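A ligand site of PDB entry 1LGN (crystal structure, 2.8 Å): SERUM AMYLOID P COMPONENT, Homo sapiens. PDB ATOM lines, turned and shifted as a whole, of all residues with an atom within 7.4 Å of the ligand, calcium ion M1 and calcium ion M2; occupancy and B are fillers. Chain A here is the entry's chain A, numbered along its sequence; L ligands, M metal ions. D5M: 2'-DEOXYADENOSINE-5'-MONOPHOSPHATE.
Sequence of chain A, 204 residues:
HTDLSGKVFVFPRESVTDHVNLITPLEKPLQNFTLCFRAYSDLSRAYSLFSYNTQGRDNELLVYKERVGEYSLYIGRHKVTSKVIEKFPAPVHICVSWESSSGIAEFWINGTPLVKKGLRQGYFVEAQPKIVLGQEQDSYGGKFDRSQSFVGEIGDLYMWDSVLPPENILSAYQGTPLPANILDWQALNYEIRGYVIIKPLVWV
Five residues have an atom within 4 Å of calcium ion M1: Asp 58, Asn 59, Glu 136, Gln 137 and Asp 138.
The nearest printed residue that does not touch calcium ion M1 is Asn 53 (5.0 Å).
A nitrogen (N6) of the ligand lies within hydrogen-bond range of the side-chain hydroxyl of Ser 147.
The side-chain hydroxyl (OH) of Tyr 74 sits at hydrogen-bond distance from an oxygen (O3') of the ligand (3.4 Å).
A nitrogen (N6) of the ligand lies within hydrogen-bond range of the side-chain carboxylate (OD1) of Asp 145.
OH of Tyr 64 lies within hydrogen-bond range of O4' of the ligand (3.2 Å).
OD2 of Asp 138 is bound to calcium ion M2 (2.4 Å).
Calcium ion M2 is bound by an oxygen (O3P) of the ligand (2.4 Å).
The side-chain carboxylate (OE1) of Glu 136 is bound to calcium ion M2, at 2.4 Å.
OE1 of Gln 148 binds calcium ion M2, 2.4 Å away.
The side-chain carboxylate (OD1) of Asp 138 binds calcium ion M2 (2.7 Å).
Calcium ion M2 has five donor atoms within binding distance.
Merely in contact with calcium ion M2: Asp 145 (3.8 Å).
Within 4 Å of calcium ion M2: Glu 136, Asp 138, Asp 145 and Gln 148.
Nine residues have an atom within 4 Å of the ligand: Asp 58, Asn 59, Tyr 64, Tyr 74, Glu 136, Asp 138, Asp 145, Ser 147 and Gln 148.
Along chain A the residues within 4 Å of the ligand span positions 58 to 148.
The nearest printed residue that does not touch the ligand is Lys 79 (4.3 Å).
Calcium ion M1 is bound by O2P of the ligand (2.3 Å), OE2 of Glu 136 (2.3 Å), OD1 of Asn 59 (2.3 Å), OD1 of Asp 138 (2.4 Å), OD1 of Asp 58 (2.5 Å), O of Gln 137 (2.5 Å), OE1 of Glu 136 (2.9 Å) and OD2 of Asp 58 (2.9 Å).
Calcium ion M1 has eight donor atoms within binding distance.
The backbone carbonyl oxygen (O) of Lys 143 sits close to the backbone NH (N) of Asp 138 (3.4 Å).
NE2 of Gln 148 sits at hydrogen-bond distance from OH of Tyr 64 (2.7 Å).
OD1 of Asp 145 sits at hydrogen-bond distance from OG of Ser 147.
The backbone NH (N) of Asn 59 is in hydrogen-bond range of the side-chain amide oxygen (OD1) of Asn 53 (3.1 Å).
The backbone NH (N) of Gln 137 lies within hydrogen-bond range of the side-chain hydroxyl (OG) of Ser 51, at 3.3 Å.
OE1 of Gln 137 sits close to O of Ser 139.
The side-chain carboxylate (OD1) of Asp 58 sits close to the side-chain amide nitrogen (ND2) of Asn 53.
N of Tyr 74 is in hydrogen-bond range of O of Leu 62 (2.9 Å).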
ATOM      1  N   ALA A  46     -20.094 -23.752 -20.020  1.00  0.00           N
ATOM      2  CA  ALA A  46     -19.562 -25.076 -20.288  1.00  0.00           C
ATOM      3  C   ALA A  46     -18.439 -25.298 -19.309  1.00  0.00           C
ATOM      4  O   ALA A  46     -17.815 -24.349 -18.823  1.00  0.00           O
ATOM      5  CB  ALA A  46     -19.043 -25.159 -21.692  1.00  0.00           C
ATOM      6  N   SER A  51     -10.936 -34.642 -17.087  1.00  0.00           N
ATOM      7  CA  SER A  51      -9.897 -34.471 -18.104  1.00  0.00           C
ATOM      8  C   SER A  51      -8.838 -35.560 -17.995  1.00  0.00           C
ATOM      9  O   SER A  51      -8.398 -35.893 -16.905  1.00  0.00           O
ATOM     10  CB  SER A  51      -9.256 -33.083 -17.968  1.00  0.00           C
ATOM     11  OG  SER A  51      -8.503 -32.733 -19.120  1.00  0.00           O
ATOM     12  N   ASN A  53      -5.296 -36.509 -20.202  1.00  0.00           N
ATOM     13  CA  ASN A  53      -4.336 -36.244 -21.263  1.00  0.00           C
ATOM     14  C   ASN A  53      -3.088 -37.094 -21.096  1.00  0.00           C
ATOM     15  O   ASN A  53      -2.706 -37.429 -19.979  1.00  0.00           O
ATOM     16  CB  ASN A  53      -3.876 -34.785 -21.242  1.00  0.00           C
ATOM     17  CG  ASN A  53      -4.845 -33.869 -21.913  1.00  0.00           C
ATOM     18  OD1 ASN A  53      -6.018 -34.188 -22.084  1.00  0.00           O
ATOM     19  ND2 ASN A  53      -4.346 -32.695 -22.310  1.00  0.00           N
ATOM     20  N   ASP A  58      -3.711 -33.972 -26.624  1.00  0.00           N
ATOM     21  CA  ASP A  58      -4.705 -33.209 -25.888  1.00  0.00           C
ATOM     22  C   ASP A  58      -6.073 -33.876 -26.056  1.00  0.00           C
ATOM     23  O   ASP A  58      -6.361 -34.439 -27.090  1.00  0.00           O
ATOM     24  CB  ASP A  58      -4.756 -31.775 -26.419  1.00  0.00           C
ATOM     25  CG  ASP A  58      -5.718 -30.870 -25.645  1.00  0.00           C
ATOM     26  OD1 ASP A  58      -5.996 -31.132 -24.456  1.00  0.00           O
ATOM     27  OD2 ASP A  58      -6.190 -29.867 -26.210  1.00  0.00           O
ATOM     28  N   ASN A  59      -6.902 -33.801 -25.026  1.00  0.00           N
ATOM     29  CA  ASN A  59      -8.230 -34.406 -25.061  1.00  0.00           C
ATOM     30  C   ASN A  59      -8.131 -35.852 -25.522  1.00  0.00           C
ATOM     31  O   ASN A  59      -8.680 -36.223 -26.550  1.00  0.00           O
ATOM     32  CB  ASN A  59      -9.157 -33.630 -25.995  1.00  0.00           C
ATOM     33  CG  ASN A  59      -9.209 -32.138 -25.694  1.00  0.00           C
ATOM     34  OD1 ASN A  59      -8.944 -31.699 -24.571  1.00  0.00           O
ATOM     35  ND2 ASN A  59      -9.523 -31.345 -26.706  1.00  0.00           N
ATOM     36  N   GLU A  60      -7.369 -36.661 -24.785  1.00  0.00           N
ATOM     37  CA  GLU A  60      -7.241 -38.061 -25.141  1.00  0.00           C
ATOM     38  C   GLU A  60      -8.520 -38.744 -24.686  1.00  0.00           C
ATOM     39  O   GLU A  60      -9.029 -39.625 -25.356  1.00  0.00           O
ATOM     40  CB  GLU A  60      -5.997 -38.675 -24.496  1.00  0.00           C
ATOM     41  CG  GLU A  60      -5.737 -40.123 -24.888  1.00  0.00           C
ATOM     42  CD  GLU A  60      -5.426 -40.302 -26.366  1.00  0.00           C
ATOM     43  OE1 GLU A  60      -5.205 -39.304 -27.064  1.00  0.00           O
ATOM     44  OE2 GLU A  60      -5.397 -41.454 -26.820  1.00  0.00           O
ATOM     45  N   LEU A  62     -11.880 -37.007 -22.593  1.00  0.00           N
ATOM     46  CA  LEU A  62     -12.489 -35.839 -21.917  1.00  0.00           C
ATOM     47  C   LEU A  62     -14.011 -35.916 -21.872  1.00  0.00           C
ATOM     48  O   LEU A  62     -14.646 -36.143 -22.892  1.00  0.00           O
ATOM     49  CB  LEU A  62     -12.078 -34.555 -22.657  1.00  0.00           C
ATOM     50  CG  LEU A  62     -12.827 -33.242 -22.481  1.00  0.00           C
ATOM     51  CD1 LEU A  62     -12.726 -32.780 -21.079  1.00  0.00           C
ATOM     52  CD2 LEU A  62     -12.242 -32.176 -23.406  1.00  0.00           C
ATOM     53  N   TYR A  64     -16.873 -33.625 -21.333  1.00  0.00           N
ATOM     54  CA  TYR A  64     -17.147 -32.195 -21.302  1.00  0.00           C
ATOM     55  C   TYR A  64     -18.628 -31.874 -21.351  1.00  0.00           C
ATOM     56  O   TYR A  64     -19.364 -32.552 -22.060  1.00  0.00           O
ATOM     57  CB  TYR A  64     -16.476 -31.580 -22.514  1.00  0.00           C
ATOM     58  CG  TYR A  64     -16.294 -30.100 -22.509  1.00  0.00           C
ATOM     59  CD1 TYR A  64     -15.350 -29.485 -21.685  1.00  0.00           C
ATOM     60  CD2 TYR A  64     -16.983 -29.311 -23.404  1.00  0.00           C
ATOM     61  CE1 TYR A  64     -15.098 -28.118 -21.761  1.00  0.00           C
ATOM     62  CE2 TYR A  64     -16.745 -27.948 -23.481  1.00  0.00           C
ATOM     63  CZ  TYR A  64     -15.800 -27.362 -22.665  1.00  0.00           C
ATOM     64  OH  TYR A  64     -15.546 -26.029 -22.793  1.00  0.00           O
ATOM     65  N   GLU A  66     -21.260 -29.259 -22.573  1.00  0.00           N
ATOM     66  CA  GLU A  66     -21.514 -28.138 -23.474  1.00  0.00           C
ATOM     67  C   GLU A  66     -22.455 -27.065 -22.945  1.00  0.00           C
ATOM     68  O   GLU A  66     -22.199 -25.871 -23.073  1.00  0.00           O
ATOM     69  CB  GLU A  66     -22.119 -28.697 -24.757  1.00  0.00           C
ATOM     70  CG  GLU A  66     -21.240 -29.726 -25.439  1.00  0.00           C
ATOM     71  CD  GLU A  66     -19.952 -29.126 -25.965  1.00  0.00           C
ATOM     72  OE1 GLU A  66     -19.900 -27.881 -26.168  1.00  0.00           O
ATOM     73  OE2 GLU A  66     -18.989 -29.896 -26.189  1.00  0.00           O
ATOM     74  N   TYR A  74     -14.899 -36.997 -25.692  1.00  0.00           N
ATOM     75  CA  TYR A  74     -13.799 -36.911 -26.636  1.00  0.00           C
ATOM     76  C   TYR A  74     -12.931 -38.160 -26.480  1.00  0.00           C
ATOM     77  O   TYR A  74     -12.655 -38.587 -25.357  1.00  0.00           O
ATOM     78  CB  TYR A  74     -12.929 -35.716 -26.332  1.00  0.00           C
ATOM     79  CG  TYR A  74     -13.463 -34.370 -26.722  1.00  0.00           C
ATOM     80  CD1 TYR A  74     -14.533 -33.778 -26.039  1.00  0.00           C
ATOM     81  CD2 TYR A  74     -12.857 -33.633 -27.756  1.00  0.00           C
ATOM     82  CE1 TYR A  74     -14.979 -32.486 -26.357  1.00  0.00           C
ATOM     83  CE2 TYR A  74     -13.302 -32.345 -28.084  1.00  0.00           C
ATOM     84  CZ  TYR A  74     -14.357 -31.782 -27.384  1.00  0.00           C
ATOM     85  OH  TYR A  74     -14.804 -30.514 -27.702  1.00  0.00           O
ATOM     86  N   LYS A  79     -14.906 -36.223 -31.136  1.00  0.00           N
ATOM     87  CA  LYS A  79     -15.995 -35.930 -30.224  1.00  0.00           C
ATOM     88  C   LYS A  79     -17.396 -36.371 -30.604  1.00  0.00           C
ATOM     89  O   LYS A  79     -17.761 -36.380 -31.778  1.00  0.00           O
ATOM     90  CB  LYS A  79     -15.977 -34.421 -30.055  1.00  0.00           C
ATOM     91  CG  LYS A  79     -17.147 -33.787 -29.394  1.00  0.00           C
ATOM     92  CD  LYS A  79     -17.077 -32.298 -29.644  1.00  0.00           C
ATOM     93  CE  LYS A  79     -18.009 -31.549 -28.714  1.00  0.00           C
ATOM     94  NZ  LYS A  79     -18.010 -30.092 -29.003  1.00  0.00           N
ATOM     95  N   GLN A 135     -10.451 -28.854 -13.726  1.00  0.00           N
ATOM     96  CA  GLN A 135      -9.855 -28.006 -14.747  1.00  0.00           C
ATOM     97  C   GLN A 135      -9.794 -28.784 -16.054  1.00  0.00           C
ATOM     98  O   GLN A 135     -10.029 -29.997 -16.070  1.00  0.00           O
ATOM     99  CB  GLN A 135      -8.442 -27.606 -14.357  1.00  0.00           C
ATOM    100  CG  GLN A 135      -8.362 -26.674 -13.192  1.00  0.00           C
ATOM    101  CD  GLN A 135      -9.008 -25.353 -13.474  1.00  0.00           C
ATOM    102  OE1 GLN A 135      -9.183 -24.969 -14.641  1.00  0.00           O
ATOM    103  NE2 GLN A 135      -9.381 -24.661 -12.416  1.00  0.00           N
ATOM    104  N   GLU A 136      -9.528 -28.091 -17.148  1.00  0.00           N
ATOM    105  CA  GLU A 136      -9.437 -28.767 -18.433  1.00  0.00           C
ATOM    106  C   GLU A 136      -8.029 -28.560 -18.945  1.00  0.00           C
ATOM    107  O   GLU A 136      -7.587 -27.420 -19.200  1.00  0.00           O
ATOM    108  CB  GLU A 136     -10.497 -28.223 -19.410  1.00  0.00           C
ATOM    109  CG  GLU A 136     -10.818 -29.135 -20.596  1.00  0.00           C
ATOM    110  CD  GLU A 136      -9.763 -29.096 -21.703  1.00  0.00           C
ATOM    111  OE1 GLU A 136      -9.339 -27.991 -22.111  1.00  0.00           O
ATOM    112  OE2 GLU A 136      -9.363 -30.180 -22.181  1.00  0.00           O
ATOM    113  N   GLN A 137      -7.310 -29.664 -19.045  1.00  0.00           N
ATOM    114  CA  GLN A 137      -5.923 -29.620 -19.495  1.00  0.00           C
ATOM    115  C   GLN A 137      -5.823 -29.343 -20.973  1.00  0.00           C
ATOM    116  O   GLN A 137      -6.650 -29.804 -21.753  1.00  0.00           O
ATOM    117  CB  GLN A 137      -5.237 -30.954 -19.245  1.00  0.00           C
ATOM    118  CG  GLN A 137      -5.110 -31.382 -17.819  1.00  0.00           C
ATOM    119  CD  GLN A 137      -4.737 -32.848 -17.719  1.00  0.00           C
ATOM    120  OE1 GLN A 137      -3.619 -33.231 -18.071  1.00  0.00           O
ATOM    121  NE2 GLN A 137      -5.672 -33.683 -17.254  1.00  0.00           N
ATOM    122  N   ASP A 138      -4.817 -28.581 -21.348  1.00  0.00           N
ATOM    123  CA  ASP A 138      -4.534 -28.302 -22.745  1.00  0.00           C
ATOM    124  C   ASP A 138      -3.088 -28.700 -22.988  1.00  0.00           C
ATOM    125  O   ASP A 138      -2.530 -28.493 -24.056  1.00  0.00           O
ATOM    126  CB  ASP A 138      -4.777 -26.846 -23.113  1.00  0.00           C
ATOM    127  CG  ASP A 138      -6.231 -26.558 -23.432  1.00  0.00           C
ATOM    128  OD1 ASP A 138      -7.012 -27.532 -23.561  1.00  0.00           O
ATOM    129  OD2 ASP A 138      -6.580 -25.354 -23.562  1.00  0.00           O
ATOM    130  N   SER A 139      -2.498 -29.301 -21.961  1.00  0.00           N
ATOM    131  CA  SER A 139      -1.136 -29.797 -21.980  1.00  0.00           C
ATOM    132  C   SER A 139      -1.117 -30.999 -21.028  1.00  0.00           C
ATOM    133  O   SER A 139      -2.144 -31.357 -20.446  1.00  0.00           O
ATOM    134  CB  SER A 139      -0.153 -28.715 -21.528  1.00  0.00           C
ATOM    135  OG  SER A 139      -0.272 -28.433 -20.150  1.00  0.00           O
ATOM    136  N   GLY A 142      -1.366 -29.639 -17.480  1.00  0.00           N
ATOM    137  CA  GLY A 142      -1.444 -28.206 -17.311  1.00  0.00           C
ATOM    138  C   GLY A 142      -2.226 -27.397 -18.340  1.00  0.00           C
ATOM    139  O   GLY A 142      -3.160 -27.895 -18.973  1.00  0.00           O
ATOM    140  N   LYS A 143      -1.826 -26.136 -18.480  1.00  0.00           N
ATOM    141  CA  LYS A 143      -2.449 -25.164 -19.374  1.00  0.00           C
ATOM    142  C   LYS A 143      -3.969 -25.126 -19.217  1.00  0.00           C
ATOM    143  O   LYS A 143      -4.721 -25.406 -20.150  1.00  0.00           O
ATOM    144  CB  LYS A 143      -2.030 -25.390 -20.825  1.00  0.00           C
ATOM    145  N   PHE A 144      -4.399 -24.752 -18.016  1.00  0.00           N
ATOM    146  CA  PHE A 144      -5.804 -24.655 -17.647  1.00  0.00           C
ATOM    147  C   PHE A 144      -6.481 -23.399 -18.182  1.00  0.00           C
ATOM    148  O   PHE A 144      -5.867 -22.327 -18.235  1.00  0.00           O
ATOM    149  CB  PHE A 144      -5.934 -24.697 -16.128  1.00  0.00           C
ATOM    150  CG  PHE A 144      -5.405 -25.954 -15.514  1.00  0.00           C
ATOM    151  CD1 PHE A 144      -5.296 -27.119 -16.262  1.00  0.00           C
ATOM    152  CD2 PHE A 144      -5.018 -25.975 -14.188  1.00  0.00           C
ATOM    153  CE1 PHE A 144      -4.822 -28.281 -15.689  1.00  0.00           C
ATOM    154  CE2 PHE A 144      -4.544 -27.137 -13.615  1.00  0.00           C
ATOM    155  CZ  PHE A 144      -4.445 -28.294 -14.358  1.00  0.00           C
ATOM    156  N   ASP A 145      -7.748 -23.561 -18.586  1.00  0.00           N
ATOM    157  CA  ASP A 145      -8.554 -22.449 -19.060  1.00  0.00           C
ATOM    158  C   ASP A 145      -9.779 -22.272 -18.157  1.00  0.00           C
ATOM    159  O   ASP A 145     -10.639 -23.181 -18.115  1.00  0.00           O
ATOM    160  CB  ASP A 145      -8.921 -22.622 -20.536  1.00  0.00           C
ATOM    161  CG  ASP A 145      -9.216 -21.285 -21.200  1.00  0.00           C
ATOM    162  OD1 ASP A 145     -10.146 -20.589 -20.724  1.00  0.00           O
ATOM    163  OD2 ASP A 145      -8.537 -20.936 -22.184  1.00  0.00           O
ATOM    164  N   ARG A 146      -9.721 -21.099 -17.500  1.00  0.00           N
ATOM    165  CA  ARG A 146     -10.655 -20.602 -16.484  1.00  0.00           C
ATOM    166  C   ARG A 146     -12.084 -20.713 -16.890  1.00  0.00           C
ATOM    167  O   ARG A 146     -12.936 -21.020 -16.051  1.00  0.00           O
ATOM    168  CB  ARG A 146     -10.381 -19.118 -16.122  1.00  0.00           C
ATOM    169  CG  ARG A 146     -11.420 -18.539 -15.160  1.00  0.00           C
ATOM    170  CD  ARG A 146     -11.318 -17.016 -15.042  1.00  0.00           C
ATOM    171  NE  ARG A 146     -10.619 -16.607 -13.832  1.00  0.00           N
ATOM    172  CZ  ARG A 146     -11.183 -16.485 -12.631  1.00  0.00           C
ATOM    173  NH1 ARG A 146     -12.470 -16.747 -12.454  1.00  0.00           N
ATOM    174  NH2 ARG A 146     -10.442 -16.092 -11.585  1.00  0.00           N
ATOM    175  N   SER A 147     -12.348 -20.455 -18.143  1.00  0.00           N
ATOM    176  CA  SER A 147     -13.695 -20.515 -18.640  1.00  0.00           C
ATOM    177  C   SER A 147     -14.189 -21.952 -18.821  1.00  0.00           C
ATOM    178  O   SER A 147     -15.305 -22.178 -19.273  1.00  0.00           O
ATOM    179  CB  SER A 147     -13.833 -19.738 -19.954  1.00  0.00           C
ATOM    180  OG  SER A 147     -12.774 -20.055 -20.847  1.00  0.00           O
ATOM    181  N   GLN A 148     -13.345 -22.911 -18.470  1.00  0.00           N
ATOM    182  CA  GLN A 148     -13.717 -24.315 -18.560  1.00  0.00           C
ATOM    183  C   GLN A 148     -13.642 -24.972 -17.200  1.00  0.00           C
ATOM    184  O   GLN A 148     -13.979 -26.141 -17.074  1.00  0.00           O
ATOM    185  CB  GLN A 148     -12.821 -25.064 -19.551  1.00  0.00           C
ATOM    186  CG  GLN A 148     -13.031 -24.602 -20.960  1.00  0.00           C
ATOM    187  CD  GLN A 148     -12.199 -25.358 -21.946  1.00  0.00           C
ATOM    188  OE1 GLN A 148     -10.987 -25.489 -21.779  1.00  0.00           O
ATOM    189  NE2 GLN A 148     -12.836 -25.834 -23.004  1.00  0.00           N
HETATM  190  O5' D5M L   1     -11.359 -27.611 -26.393  1.00  0.00           O
HETATM  191  C5' D5M L   1     -12.457 -28.212 -25.750  1.00  0.00           C
HETATM  192  C4' D5M L   1     -13.724 -27.493 -26.225  1.00  0.00           C
HETATM  193  O4' D5M L   1     -13.924 -26.266 -25.497  1.00  0.00           O
HETATM  194  C3' D5M L   1     -13.608 -27.094 -27.681  1.00  0.00           C
HETATM  195  O3' D5M L   1     -14.895 -27.156 -28.247  1.00  0.00           O
HETATM  196  C2' D5M L   1     -13.220 -25.642 -27.667  1.00  0.00           C
HETATM  197  C1' D5M L   1     -13.853 -25.150 -26.395  1.00  0.00           C
HETATM  198  N9  D5M L   1     -12.998 -24.165 -25.759  1.00  0.00           N
HETATM  199  C8  D5M L   1     -11.672 -24.206 -25.496  1.00  0.00           C
HETATM  200  N7  D5M L   1     -11.186 -23.163 -24.895  1.00  0.00           N
HETATM  201  C5  D5M L   1     -12.279 -22.351 -24.743  1.00  0.00           C
HETATM  202  C6  D5M L   1     -12.446 -21.077 -24.165  1.00  0.00           C
HETATM  203  N6  D5M L   1     -11.463 -20.386 -23.596  1.00  0.00           N
HETATM  204  N1  D5M L   1     -13.692 -20.523 -24.192  1.00  0.00           N
HETATM  205  C2  D5M L   1     -14.680 -21.223 -24.758  1.00  0.00           C
HETATM  206  N3  D5M L   1     -14.641 -22.458 -25.317  1.00  0.00           N
HETATM  207  C4  D5M L   1     -13.397 -22.955 -25.273  1.00  0.00           C
HETATM  208  P   D5M L   1      -9.925 -27.448 -25.743  1.00  0.00           P
HETATM  209  O1P D5M L   1      -9.136 -26.784 -26.827  1.00  0.00           O
HETATM  210  O3P D5M L   1      -9.994 -26.561 -24.522  1.00  0.00           O
HETATM  211  O2P D5M L   1      -9.473 -28.862 -25.410  1.00  0.00           O
HETATM  212 CA    CA M   1      -7.935 -29.680 -23.935  1.00  0.00          CA
HETATM  213 CA    CA M   2      -8.733 -25.714 -22.669  1.00  0.00          CA
